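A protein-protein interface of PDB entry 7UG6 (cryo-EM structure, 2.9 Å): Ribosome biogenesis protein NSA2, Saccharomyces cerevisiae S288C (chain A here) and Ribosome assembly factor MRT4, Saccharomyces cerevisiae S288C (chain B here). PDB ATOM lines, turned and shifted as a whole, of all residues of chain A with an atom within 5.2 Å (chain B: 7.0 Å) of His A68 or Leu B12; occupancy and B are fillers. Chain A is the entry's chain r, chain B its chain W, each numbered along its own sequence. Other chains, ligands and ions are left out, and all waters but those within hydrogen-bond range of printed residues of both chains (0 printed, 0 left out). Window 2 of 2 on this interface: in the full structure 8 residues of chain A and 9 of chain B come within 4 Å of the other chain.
The backbone carbonyl oxygen (O) of Ala B13 is in hydrogen-bond range of a ring nitrogen (NE2) of His A68 (3.4 Å).
O of Ala B13 lies within hydrogen-bond range of NZ of Lys A72.
The side-chain amino group (NZ) of Lys A72 lies within hydrogen-bond range of the backbone carbonyl oxygen (O) of Gln B14 (3.4 Å).
The side-chain amino group (NZ) of Lys A72 lies within salt-bridge range of the side-chain carboxylate (OD1) of Asp B16.
CG of Lys A64 touches CD1 of Leu B12, at 3.6 Å.
Ile A65 touches Leu B12.
His A68 touches Leu B12 (CE1 to C, 3.6 Å).
The backbone carbonyl oxygen (O) of Ile A65 lies close to the side-chain carboxylate (OE1) of Glu A69, at 2.5 Å.
OG of Ser A71 lies within hydrogen-bond range of O of His A68 (2.4 Å).
Printed residues of chain B within 4 Å of Lys A64: Leu B12 (3.6 Å).
Lys A66 touches none of the printed residues of chain B.
Ala A67 touches none of the printed residues of chain B.
Of the printed residues of chain B, His A68 touches Leu B12 (3.6 Å) and Ala B13 (3.4 Å).
Leu B12 touches three residues of chain A.
Of the printed residues of chain A, Ala B13 touches His A68 and Lys A72.
The nearest residue of chain A that does not touch Leu B12 is Met A61 (5.1 Å).
The nearest printed residue of chain B that does not touch Ile A65 is Val B10 (4.6 Å).
Of the 11 printed residues of chain A, 4 touch a printed residue of chain B.
Hydrophobic or aromatic side chains of chain A that line the printed part of chain B: Ile A65 and His A68.
Among the printed residues, 7 pairs touch across the chains.
Among the printed residues, Asp or Glu carboxylates within 4 Å of a Lys or Arg side-chain nitrogen of the other chain: Lys A72 with Asp B16.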
ATOM      1  N   MET A  61      -0.309 -11.838  17.589  1.00  0.00           N
ATOM      2  CA  MET A  61      -1.732 -11.584  17.786  1.00  0.00           C
ATOM      3  C   MET A  61      -2.326 -12.545  18.795  1.00  0.00           C
ATOM      4  O   MET A  61      -3.114 -12.143  19.657  1.00  0.00           O
ATOM      5  CB  MET A  61      -2.479 -11.687  16.464  1.00  0.00           C
ATOM      6  CG  MET A  61      -3.931 -11.292  16.574  1.00  0.00           C
ATOM      7  SD  MET A  61      -4.159  -9.557  16.974  1.00  0.00           S
ATOM      8  CE  MET A  61      -5.787  -9.593  17.713  1.00  0.00           C
ATOM      9  N   LYS A  63      -0.735 -14.055  21.245  1.00  0.00           N
ATOM     10  CA  LYS A  63      -0.247 -13.733  22.579  1.00  0.00           C
ATOM     11  C   LYS A  63      -0.914 -12.477  23.113  1.00  0.00           C
ATOM     12  O   LYS A  63      -1.238 -12.404  24.300  1.00  0.00           O
ATOM     13  CB  LYS A  63       1.270 -13.596  22.562  1.00  0.00           C
ATOM     14  CG  LYS A  63       1.973 -14.941  22.508  1.00  0.00           C
ATOM     15  CD  LYS A  63       3.463 -14.822  22.226  1.00  0.00           C
ATOM     16  CE  LYS A  63       4.250 -14.428  23.452  1.00  0.00           C
ATOM     17  NZ  LYS A  63       5.716 -14.418  23.177  1.00  0.00           N
ATOM     18  N   LYS A  64      -1.141 -11.486  22.246  1.00  0.00           N
ATOM     19  CA  LYS A  64      -1.898 -10.299  22.630  1.00  0.00           C
ATOM     20  C   LYS A  64      -3.273 -10.667  23.151  1.00  0.00           C
ATOM     21  O   LYS A  64      -3.687 -10.211  24.223  1.00  0.00           O
ATOM     22  CB  LYS A  64      -2.045  -9.365  21.441  1.00  0.00           C
ATOM     23  CG  LYS A  64      -2.720  -8.064  21.773  1.00  0.00           C
ATOM     24  CD  LYS A  64      -2.861  -7.184  20.543  1.00  0.00           C
ATOM     25  CE  LYS A  64      -1.532  -6.615  20.084  1.00  0.00           C
ATOM     26  NZ  LYS A  64      -0.974  -5.641  21.060  1.00  0.00           N
ATOM     27  N   ILE A  65      -4.000 -11.488  22.392  1.00  0.00           N
ATOM     28  CA  ILE A  65      -5.286 -11.986  22.856  1.00  0.00           C
ATOM     29  C   ILE A  65      -5.135 -12.619  24.226  1.00  0.00           C
ATOM     30  O   ILE A  65      -5.613 -12.076  25.227  1.00  0.00           O
ATOM     31  CB  ILE A  65      -5.855 -12.984  21.838  1.00  0.00           C
ATOM     32  CG1 ILE A  65      -6.206 -12.297  20.529  1.00  0.00           C
ATOM     33  CG2 ILE A  65      -7.079 -13.657  22.378  1.00  0.00           C
ATOM     34  CD1 ILE A  65      -7.421 -11.461  20.609  1.00  0.00           C
ATOM     35  N   LYS A  66      -4.354 -13.693  24.306  1.00  0.00           N
ATOM     36  CA  LYS A  66      -4.291 -14.503  25.515  1.00  0.00           C
ATOM     37  C   LYS A  66      -3.926 -13.666  26.728  1.00  0.00           C
ATOM     38  O   LYS A  66      -4.489 -13.856  27.811  1.00  0.00           O
ATOM     39  CB  LYS A  66      -3.288 -15.630  25.315  1.00  0.00           C
ATOM     40  CG  LYS A  66      -3.198 -16.593  26.459  1.00  0.00           C
ATOM     41  CD  LYS A  66      -2.370 -17.782  26.050  1.00  0.00           C
ATOM     42  CE  LYS A  66      -3.250 -18.816  25.397  1.00  0.00           C
ATOM     43  NZ  LYS A  66      -4.223 -19.365  26.373  1.00  0.00           N
ATOM     44  N   ALA A  67      -3.038 -12.692  26.550  1.00  0.00           N
ATOM     45  CA  ALA A  67      -2.736 -11.762  27.628  1.00  0.00           C
ATOM     46  C   ALA A  67      -3.947 -10.916  27.987  1.00  0.00           C
ATOM     47  O   ALA A  67      -4.189 -10.648  29.166  1.00  0.00           O
ATOM     48  CB  ALA A  67      -1.557 -10.876  27.241  1.00  0.00           C
ATOM     49  N   HIS A  68      -4.726 -10.487  26.991  1.00  0.00           N
ATOM     50  CA  HIS A  68      -5.899  -9.664  27.281  1.00  0.00           C
ATOM     51  C   HIS A  68      -6.927 -10.422  28.114  1.00  0.00           C
ATOM     52  O   HIS A  68      -7.351  -9.953  29.181  1.00  0.00           O
ATOM     53  CB  HIS A  68      -6.528  -9.177  25.982  1.00  0.00           C
ATOM     54  CG  HIS A  68      -7.953  -8.756  26.125  1.00  0.00           C
ATOM     55  ND1 HIS A  68      -8.327  -7.628  26.818  1.00  0.00           N
ATOM     56  CD2 HIS A  68      -9.096  -9.318  25.672  1.00  0.00           C
ATOM     57  CE1 HIS A  68      -9.640  -7.510  26.781  1.00  0.00           C
ATOM     58  NE2 HIS A  68     -10.132  -8.523  26.092  1.00  0.00           N
ATOM     59  N   GLU A  69      -7.333 -11.606  27.651  1.00  0.00           N
ATOM     60  CA  GLU A  69      -8.292 -12.371  28.453  1.00  0.00           C
ATOM     61  C   GLU A  69      -7.720 -12.785  29.802  1.00  0.00           C
ATOM     62  O   GLU A  69      -8.431 -12.737  30.810  1.00  0.00           O
ATOM     63  CB  GLU A  69      -8.882 -13.580  27.714  1.00  0.00           C
ATOM     64  CG  GLU A  69      -9.817 -13.235  26.547  1.00  0.00           C
ATOM     65  CD  GLU A  69      -9.104 -12.940  25.276  1.00  0.00           C
ATOM     66  OE1 GLU A  69      -7.890 -13.080  25.303  1.00  0.00           O
ATOM     67  OE2 GLU A  69      -9.740 -12.538  24.275  1.00  0.00           O
ATOM     68  N   GLN A  70      -6.447 -13.173  29.869  1.00  0.00           N
ATOM     69  CA  GLN A  70      -5.913 -13.525  31.177  1.00  0.00           C
ATOM     70  C   GLN A  70      -5.775 -12.294  32.073  1.00  0.00           C
ATOM     71  O   GLN A  70      -5.691 -12.430  33.295  1.00  0.00           O
ATOM     72  CB  GLN A  70      -4.582 -14.264  31.007  1.00  0.00           C
ATOM     73  CG  GLN A  70      -3.954 -14.768  32.296  1.00  0.00           C
ATOM     74  CD  GLN A  70      -4.783 -15.863  32.956  1.00  0.00           C
ATOM     75  OE1 GLN A  70      -5.312 -16.748  32.284  1.00  0.00           O
ATOM     76  NE2 GLN A  70      -4.905 -15.800  34.277  1.00  0.00           N
ATOM     77  N   SER A  71      -5.781 -11.097  31.496  1.00  0.00           N
ATOM     78  CA  SER A  71      -5.848  -9.892  32.307  1.00  0.00           C
ATOM     79  C   SER A  71      -7.247  -9.635  32.836  1.00  0.00           C
ATOM     80  O   SER A  71      -7.400  -9.163  33.965  1.00  0.00           O
ATOM     81  CB  SER A  71      -5.381  -8.684  31.499  1.00  0.00           C
ATOM     82  OG  SER A  71      -6.407  -8.242  30.628  1.00  0.00           O
ATOM     83  N   LYS A  72      -8.279  -9.919  32.042  1.00  0.00           N
ATOM     84  CA  LYS A  72      -9.627  -9.624  32.516  1.00  0.00           C
ATOM     85  C   LYS A  72     -10.171 -10.691  33.454  1.00  0.00           C
ATOM     86  O   LYS A  72     -11.192 -10.455  34.104  1.00  0.00           O
ATOM     87  CB  LYS A  72     -10.593  -9.459  31.349  1.00  0.00           C
ATOM     88  CG  LYS A  72     -11.047 -10.771  30.742  1.00  0.00           C
ATOM     89  CD  LYS A  72     -12.287 -10.577  29.897  1.00  0.00           C
ATOM     90  CE  LYS A  72     -11.985  -9.783  28.653  1.00  0.00           C
ATOM     91  NZ  LYS A  72     -13.178  -9.697  27.777  1.00  0.00           N
ATOM     92  N   VAL B  10     -12.153  -8.895  15.850  1.00  0.00           N
ATOM     93  CA  VAL B  10     -12.334  -8.824  17.290  1.00  0.00           C
ATOM     94  C   VAL B  10     -11.390  -7.771  17.841  1.00  0.00           C
ATOM     95  O   VAL B  10     -10.323  -7.515  17.279  1.00  0.00           O
ATOM     96  CB  VAL B  10     -12.085 -10.178  17.983  1.00  0.00           C
ATOM     97  CG1 VAL B  10     -13.195 -11.149  17.659  1.00  0.00           C
ATOM     98  CG2 VAL B  10     -10.746 -10.737  17.560  1.00  0.00           C
ATOM     99  N   THR B  11     -11.793  -7.149  18.946  1.00  0.00           N
ATOM    100  CA  THR B  11     -10.907  -6.237  19.645  1.00  0.00           C
ATOM    101  C   THR B  11     -10.861  -6.617  21.113  1.00  0.00           C
ATOM    102  O   THR B  11     -11.573  -7.512  21.574  1.00  0.00           O
ATOM    103  CB  THR B  11     -11.323  -4.773  19.495  1.00  0.00           C
ATOM    104  OG1 THR B  11     -10.261  -3.936  19.972  1.00  0.00           O
ATOM    105  CG2 THR B  11     -12.537  -4.494  20.318  1.00  0.00           C
ATOM    106  N   LEU B  12      -9.990  -5.934  21.839  1.00  0.00           N
ATOM    107  CA  LEU B  12      -9.720  -6.261  23.227  1.00  0.00           C
ATOM    108  C   LEU B  12     -10.436  -5.272  24.141  1.00  0.00           C
ATOM    109  O   LEU B  12      -9.836  -4.399  24.760  1.00  0.00           O
ATOM    110  CB  LEU B  12      -8.219  -6.264  23.471  1.00  0.00           C
ATOM    111  CG  LEU B  12      -7.440  -6.857  22.305  1.00  0.00           C
ATOM    112  CD1 LEU B  12      -5.961  -6.637  22.491  1.00  0.00           C
ATOM    113  CD2 LEU B  12      -7.753  -8.316  22.211  1.00  0.00           C
ATOM    114  N   ALA B  13     -11.743  -5.440  24.234  1.00  0.00           N
ATOM    115  CA  ALA B  13     -12.552  -4.618  25.111  1.00  0.00           C
ATOM    116  C   ALA B  13     -12.982  -5.418  26.330  1.00  0.00           C
ATOM    117  O   ALA B  13     -12.894  -6.646  26.360  1.00  0.00           O
ATOM    118  CB  ALA B  13     -13.778  -4.078  24.381  1.00  0.00           C
ATOM    119  N   GLN B  14     -13.465  -4.696  27.338  1.00  0.00           N
ATOM    120  CA  GLN B  14     -13.750  -5.309  28.627  1.00  0.00           C
ATOM    121  C   GLN B  14     -15.083  -6.045  28.622  1.00  0.00           C
ATOM    122  O   GLN B  14     -15.144  -7.233  28.947  1.00  0.00           O
ATOM    123  CB  GLN B  14     -13.734  -4.240  29.715  1.00  0.00           C
ATOM    124  CG  GLN B  14     -12.374  -3.651  30.001  1.00  0.00           C
ATOM    125  CD  GLN B  14     -11.460  -4.637  30.680  1.00  0.00           C
ATOM    126  OE1 GLN B  14     -10.393  -4.972  30.168  1.00  0.00           O
ATOM    127  NE2 GLN B  14     -11.879  -5.120  31.842  1.00  0.00           N
ATOM    128  N   ASP B  16     -18.532  -8.046  28.029  1.00  0.00           N
ATOM    129  CA  ASP B  16     -18.788  -9.295  27.332  1.00  0.00           C
ATOM    130  C   ASP B  16     -20.263  -9.441  26.988  1.00  0.00           C
ATOM    131  O   ASP B  16     -21.130  -8.768  27.544  1.00  0.00           O
ATOM    132  CB  ASP B  16     -18.336 -10.485  28.173  1.00  0.00           C
ATOM    133  CG  ASP B  16     -16.957 -10.289  28.739  1.00  0.00           C
ATOM    134  OD1 ASP B  16     -16.118  -9.693  28.038  1.00  0.00           O
ATOM    135  OD2 ASP B  16     -16.713 -10.720  29.885  1.00  0.00           O
